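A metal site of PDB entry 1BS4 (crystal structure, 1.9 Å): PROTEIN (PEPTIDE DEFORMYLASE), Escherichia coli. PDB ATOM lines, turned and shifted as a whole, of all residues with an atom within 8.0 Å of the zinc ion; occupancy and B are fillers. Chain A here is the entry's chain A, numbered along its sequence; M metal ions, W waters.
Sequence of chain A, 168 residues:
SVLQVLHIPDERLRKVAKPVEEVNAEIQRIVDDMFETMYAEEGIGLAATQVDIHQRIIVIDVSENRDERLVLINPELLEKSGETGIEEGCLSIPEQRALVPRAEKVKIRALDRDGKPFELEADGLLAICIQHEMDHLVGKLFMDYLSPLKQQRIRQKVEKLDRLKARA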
ATOM      1  N   VAL A   5      11.331   5.819  -3.979  1.00  0.00           N
ATOM      2  CA  VAL A   5      10.305   6.338  -3.091  1.00  0.00           C
ATOM      3  C   VAL A   5      10.394   7.867  -3.062  1.00  0.00           C
ATOM      4  O   VAL A   5      11.451   8.423  -2.821  1.00  0.00           O
ATOM      5  CB  VAL A   5      10.473   5.782  -1.669  1.00  0.00           C
ATOM      6  CG1 VAL A   5       9.381   6.316  -0.747  1.00  0.00           C
ATOM      7  CG2 VAL A   5      10.446   4.271  -1.702  1.00  0.00           C
ATOM      8  N   LEU A  13       3.057  13.437  -4.162  1.00  0.00           N
ATOM      9  CA  LEU A  13       2.575  12.825  -2.931  1.00  0.00           C
ATOM     10  C   LEU A  13       1.167  13.318  -2.562  1.00  0.00           C
ATOM     11  O   LEU A  13       0.472  12.697  -1.751  1.00  0.00           O
ATOM     12  CB  LEU A  13       3.575  13.122  -1.809  1.00  0.00           C
ATOM     13  CG  LEU A  13       4.604  12.117  -1.250  1.00  0.00           C
ATOM     14  CD1 LEU A  13       4.565  10.765  -1.914  1.00  0.00           C
ATOM     15  CD2 LEU A  13       5.971  12.737  -1.347  1.00  0.00           C
ATOM     16  N   GLY A  45       5.170  -0.685   5.667  1.00  0.00           N
ATOM     17  CA  GLY A  45       4.033  -0.375   4.825  1.00  0.00           C
ATOM     18  C   GLY A  45       4.462   0.521   3.680  1.00  0.00           C
ATOM     19  O   GLY A  45       5.427   1.290   3.784  1.00  0.00           O
ATOM     20  N   LEU A  46       3.760   0.404   2.562  1.00  0.00           N
ATOM     21  CA  LEU A  46       3.992   1.245   1.399  1.00  0.00           C
ATOM     22  C   LEU A  46       2.691   1.412   0.588  1.00  0.00           C
ATOM     23  O   LEU A  46       1.907   0.482   0.443  1.00  0.00           O
ATOM     24  CB  LEU A  46       5.102   0.629   0.524  1.00  0.00           C
ATOM     25  CG  LEU A  46       5.785   1.527  -0.519  1.00  0.00           C
ATOM     26  CD1 LEU A  46       6.530   2.678   0.152  1.00  0.00           C
ATOM     27  CD2 LEU A  46       6.733   0.688  -1.329  1.00  0.00           C
ATOM     28  N   ALA A  47       2.377   2.657   0.237  1.00  0.00           N
ATOM     29  CA  ALA A  47       1.245   2.932  -0.636  1.00  0.00           C
ATOM     30  C   ALA A  47       1.763   3.187  -2.046  1.00  0.00           C
ATOM     31  O   ALA A  47       2.860   3.731  -2.216  1.00  0.00           O
ATOM     32  CB  ALA A  47       0.501   4.155  -0.144  1.00  0.00           C
ATOM     33  N   GLN A  50       3.353   6.542  -3.134  1.00  0.00           N
ATOM     34  CA  GLN A  50       4.703   6.848  -2.646  1.00  0.00           C
ATOM     35  C   GLN A  50       5.755   6.525  -3.694  1.00  0.00           C
ATOM     36  O   GLN A  50       6.855   7.079  -3.677  1.00  0.00           O
ATOM     37  CB  GLN A  50       4.997   6.065  -1.369  1.00  0.00           C
ATOM     38  CG  GLN A  50       4.336   6.646  -0.154  1.00  0.00           C
ATOM     39  CD  GLN A  50       4.666   5.876   1.074  1.00  0.00           C
ATOM     40  OE1 GLN A  50       3.976   4.920   1.436  1.00  0.00           O
ATOM     41  NE2 GLN A  50       5.760   6.256   1.729  1.00  0.00           N
ATOM     42  N   GLU A  88       4.601   7.569  14.570  1.00  0.00           N
ATOM     43  CA  GLU A  88       4.661   6.978  13.228  1.00  0.00           C
ATOM     44  C   GLU A  88       5.898   7.438  12.460  1.00  0.00           C
ATOM     45  O   GLU A  88       6.347   8.572  12.618  1.00  0.00           O
ATOM     46  CB  GLU A  88       3.411   7.369  12.457  1.00  0.00           C
ATOM     47  CG  GLU A  88       2.133   6.919  13.105  1.00  0.00           C
ATOM     48  CD  GLU A  88       0.891   7.184  12.259  1.00  0.00           C
ATOM     49  OE1 GLU A  88       1.017   7.487  11.056  1.00  0.00           O
ATOM     50  OE2 GLU A  88      -0.224   7.067  12.807  1.00  0.00           O
ATOM     51  N   GLY A  89       6.392   6.563  11.590  1.00  0.00           N
ATOM     52  CA  GLY A  89       7.339   6.966  10.580  1.00  0.00           C
ATOM     53  C   GLY A  89       6.755   6.781   9.203  1.00  0.00           C
ATOM     54  O   GLY A  89       5.602   6.390   9.053  1.00  0.00           O
ATOM     55  N   CYS A  90       7.573   7.014   8.182  1.00  0.00           N
ATOM     56  CA  CYS A  90       7.123   6.944   6.795  1.00  0.00           C
ATOM     57  C   CYS A  90       8.337   7.037   5.901  1.00  0.00           C
ATOM     58  O   CYS A  90       9.201   7.897   6.105  1.00  0.00           O
ATOM     59  CB  CYS A  90       6.163   8.109   6.494  1.00  0.00           C
ATOM     60  SG  CYS A  90       5.467   8.107   4.831  1.00  0.00           S
ATOM     61  N   LEU A  91       8.403   6.173   4.889  1.00  0.00           N
ATOM     62  CA  LEU A  91       9.557   6.151   3.998  1.00  0.00           C
ATOM     63  C   LEU A  91       9.632   7.405   3.131  1.00  0.00           C
ATOM     64  O   LEU A  91      10.710   7.762   2.633  1.00  0.00           O
ATOM     65  CB  LEU A  91       9.523   4.885   3.130  1.00  0.00           C
ATOM     66  CG  LEU A  91       9.832   3.556   3.821  1.00  0.00           C
ATOM     67  CD1 LEU A  91       9.632   2.401   2.851  1.00  0.00           C
ATOM     68  CD2 LEU A  91      11.245   3.547   4.335  1.00  0.00           C
ATOM     69  N   SER A  92       8.515   8.128   3.038  1.00  0.00           N
ATOM     70  CA  SER A  92       8.498   9.410   2.330  1.00  0.00           C
ATOM     71  C   SER A  92       8.914  10.604   3.186  1.00  0.00           C
ATOM     72  O   SER A  92       9.083  11.698   2.664  1.00  0.00           O
ATOM     73  CB  SER A  92       7.117   9.673   1.750  1.00  0.00           C
ATOM     74  OG  SER A  92       6.884   8.825   0.637  1.00  0.00           O
ATOM     75  N   ILE A  93       9.054  10.403   4.494  1.00  0.00           N
ATOM     76  CA  ILE A  93       9.457  11.471   5.387  1.00  0.00           C
ATOM     77  C   ILE A  93      10.623  10.982   6.241  1.00  0.00           C
ATOM     78  O   ILE A  93      10.481  10.683   7.428  1.00  0.00           O
ATOM     79  CB  ILE A  93       8.283  11.963   6.272  1.00  0.00           C
ATOM     80  CG1 ILE A  93       7.093  12.331   5.367  1.00  0.00           C
ATOM     81  CG2 ILE A  93       8.677  13.213   7.054  1.00  0.00           C
ATOM     82  CD1 ILE A  93       5.800  12.594   6.120  1.00  0.00           C
ATOM     83  N   ARG A 102      -5.175   8.426  15.644  1.00  0.00           N
ATOM     84  CA  ARG A 102      -5.764   7.398  14.778  1.00  0.00           C
ATOM     85  C   ARG A 102      -6.948   6.736  15.506  1.00  0.00           C
ATOM     86  O   ARG A 102      -7.038   6.799  16.729  1.00  0.00           O
ATOM     87  CB  ARG A 102      -4.736   6.304  14.460  1.00  0.00           C
ATOM     88  CG  ARG A 102      -3.508   6.770  13.683  1.00  0.00           C
ATOM     89  CD  ARG A 102      -3.859   7.182  12.256  1.00  0.00           C
ATOM     90  NE  ARG A 102      -2.640   7.484  11.529  1.00  0.00           N
ATOM     91  CZ  ARG A 102      -2.582   8.191  10.403  1.00  0.00           C
ATOM     92  NH1 ARG A 102      -3.690   8.518   9.747  1.00  0.00           N
ATOM     93  NH2 ARG A 102      -1.394   8.486   9.895  1.00  0.00           N
ATOM     94  N   CYS A 129      -1.326   1.264  10.924  1.00  0.00           N
ATOM     95  CA  CYS A 129      -0.634   1.121   9.662  1.00  0.00           C
ATOM     96  C   CYS A 129      -1.582   1.245   8.482  1.00  0.00           C
ATOM     97  O   CYS A 129      -1.285   1.947   7.515  1.00  0.00           O
ATOM     98  CB  CYS A 129       0.036  -0.243   9.632  1.00  0.00           C
ATOM     99  SG  CYS A 129       1.247  -0.314   8.387  1.00  0.00           S
ATOM    100  N   HIS A 132      -2.743   4.913   8.105  1.00  0.00           N
ATOM    101  CA  HIS A 132      -1.640   5.721   7.586  1.00  0.00           C
ATOM    102  C   HIS A 132      -1.482   5.495   6.076  1.00  0.00           C
ATOM    103  O   HIS A 132      -1.258   6.433   5.329  1.00  0.00           O
ATOM    104  CB  HIS A 132      -0.346   5.331   8.346  1.00  0.00           C
ATOM    105  CG  HIS A 132       0.907   5.899   7.752  1.00  0.00           C
ATOM    106  ND1 HIS A 132       1.803   6.622   8.493  1.00  0.00           N
ATOM    107  CD2 HIS A 132       1.440   5.783   6.514  1.00  0.00           C
ATOM    108  CE1 HIS A 132       2.835   6.954   7.730  1.00  0.00           C
ATOM    109  NE2 HIS A 132       2.636   6.452   6.524  1.00  0.00           N
ATOM    110  N   GLU A 133      -1.595   4.242   5.636  1.00  0.00           N
ATOM    111  CA  GLU A 133      -1.408   3.914   4.228  1.00  0.00           C
ATOM    112  C   GLU A 133      -2.620   4.316   3.381  1.00  0.00           C
ATOM    113  O   GLU A 133      -2.467   4.777   2.253  1.00  0.00           O
ATOM    114  CB  GLU A 133      -1.124   2.412   4.030  1.00  0.00           C
ATOM    115  CG  GLU A 133       0.212   1.943   4.612  1.00  0.00           C
ATOM    116  CD  GLU A 133       1.397   2.767   4.156  1.00  0.00           C
ATOM    117  OE1 GLU A 133       1.392   3.281   3.013  1.00  0.00           O
ATOM    118  OE2 GLU A 133       2.333   2.897   4.965  1.00  0.00           O
ATOM    119  N   ASP A 135      -4.362   6.911   4.008  1.00  0.00           N
ATOM    120  CA  ASP A 135      -4.216   8.358   3.874  1.00  0.00           C
ATOM    121  C   ASP A 135      -3.409   8.701   2.637  1.00  0.00           C
ATOM    122  O   ASP A 135      -3.739   9.641   1.937  1.00  0.00           O
ATOM    123  CB  ASP A 135      -3.497   8.953   5.088  1.00  0.00           C
ATOM    124  CG  ASP A 135      -4.450   9.449   6.158  1.00  0.00           C
ATOM    125  OD1 ASP A 135      -5.691   9.284   5.998  1.00  0.00           O
ATOM    126  OD2 ASP A 135      -3.960   9.980   7.165  1.00  0.00           O
ATOM    127  N   HIS A 136      -2.315   7.984   2.418  1.00  0.00           N
ATOM    128  CA  HIS A 136      -1.445   8.235   1.278  1.00  0.00           C
ATOM    129  C   HIS A 136      -2.201   8.293  -0.033  1.00  0.00           C
ATOM    130  O   HIS A 136      -1.916   9.150  -0.878  1.00  0.00           O
ATOM    131  CB  HIS A 136      -0.354   7.166   1.185  1.00  0.00           C
ATOM    132  CG  HIS A 136       0.833   7.429   2.057  1.00  0.00           C
ATOM    133  ND1 HIS A 136       1.596   8.578   1.949  1.00  0.00           N
ATOM    134  CD2 HIS A 136       1.423   6.679   3.020  1.00  0.00           C
ATOM    135  CE1 HIS A 136       2.611   8.506   2.791  1.00  0.00           C
ATOM    136  NE2 HIS A 136       2.531   7.368   3.464  1.00  0.00           N
ATOM    137  N   LYS A 140      -2.674  12.444   1.683  1.00  0.00           N
ATOM    138  CA  LYS A 140      -2.419  12.863   3.056  1.00  0.00           C
ATOM    139  C   LYS A 140      -1.159  12.241   3.628  1.00  0.00           C
ATOM    140  O   LYS A 140      -0.936  11.029   3.508  1.00  0.00           O
ATOM    141  CB  LYS A 140      -3.596  12.496   3.953  1.00  0.00           C
ATOM    142  CG  LYS A 140      -4.831  13.329   3.720  1.00  0.00           C
ATOM    143  CD  LYS A 140      -5.692  13.375   4.973  1.00  0.00           C
ATOM    144  CE  LYS A 140      -4.928  13.977   6.147  1.00  0.00           C
ATOM    145  NZ  LYS A 140      -5.838  14.350   7.287  1.00  0.00           N
ATOM    146  N   LEU A 141      -0.416  13.045   4.380  1.00  0.00           N
ATOM    147  CA  LEU A 141       0.789  12.617   5.080  1.00  0.00           C
ATOM    148  C   LEU A 141       0.572  12.772   6.601  1.00  0.00           C
ATOM    149  O   LEU A 141      -0.277  13.548   7.028  1.00  0.00           O
ATOM    150  CB  LEU A 141       1.962  13.478   4.619  1.00  0.00           C
ATOM    151  CG  LEU A 141       2.229  13.489   3.109  1.00  0.00           C
ATOM    152  CD1 LEU A 141       3.120  14.671   2.758  1.00  0.00           C
ATOM    153  CD2 LEU A 141       2.876  12.163   2.700  1.00  0.00           C
ATOM    154  N   PHE A 142       1.345  12.055   7.412  1.00  0.00           N
ATOM    155  CA  PHE A 142       1.089  12.090   8.852  1.00  0.00           C
ATOM    156  C   PHE A 142       1.410  13.477   9.445  1.00  0.00           C
ATOM    157  O   PHE A 142       0.746  13.906  10.386  1.00  0.00           O
ATOM    158  CB  PHE A 142       1.826  10.946   9.588  1.00  0.00           C
ATOM    159  CG  PHE A 142       3.308  11.164   9.799  1.00  0.00           C
ATOM    160  CD1 PHE A 142       3.777  12.173  10.648  1.00  0.00           C
ATOM    161  CD2 PHE A 142       4.240  10.315   9.210  1.00  0.00           C
ATOM    162  CE1 PHE A 142       5.137  12.326  10.892  1.00  0.00           C
ATOM    163  CE2 PHE A 142       5.596  10.457   9.462  1.00  0.00           C
ATOM    164  CZ  PHE A 142       6.043  11.467  10.302  1.00  0.00           C
HETATM  165 ZN    ZN M   1       3.788   6.608   4.835  1.00  0.00          ZN
HETATM  166  O   HOH W   1       3.945   4.853   4.372  1.00  0.00           O
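A ring nitrogen (NE2) of His 136 lies close to the side-chain amide oxygen (OE1) of Gln 50. A ring nitrogen (ND1) of His 132 lies within hydrogen-bond range of the side-chain carboxylate of Glu 88 (2.8 Å). SG of Cys 90 lies close to NE2 of Gln 50, 3.6 Å away. SG of Cys 90 lies close to N of Ser 92 (3.5 Å). The side-chain carboxylate of Glu 133 lies close to the side-chain amide oxygen of Gln 50 (3.4 Å). The side-chain amide nitrogen (NE2) of Gln 50 sits at hydrogen-bond distance from the side-chain hydroxyl (OG) of Ser 92 (3.0 Å). N of Ala 47 is in hydrogen-bond range of OE1 of Gln 50 (3.0 Å). The side-chain carboxylate of Glu 133 sits at hydrogen-bond distance from the backbone NH of Ala 47, at 3.0 Å.
Merely in contact with the zinc ion: Gln 50 (3.7 Å) and Glu 133 (3.99 Å). Within 4 Å of the zinc ion: Gln 50, Cys 90, His 132, Glu 133 and His 136. The nearest printed residue that does not touch the zinc ion is Gly 89 (4.6 Å).
The zinc ion is bound by water W1 (1.8 Å), NE2 of His 136 (2.0 Å), NE2 of His 132 (2.1 Å) and SG of Cys 90 (2.3 Å). The zinc ion has four donor atoms within binding distance.
Water W1 lies within hydrogen-bond range of OE2 of Glu 133 (2.6 Å) and OE1 of Gln 50 (2.9 Å).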
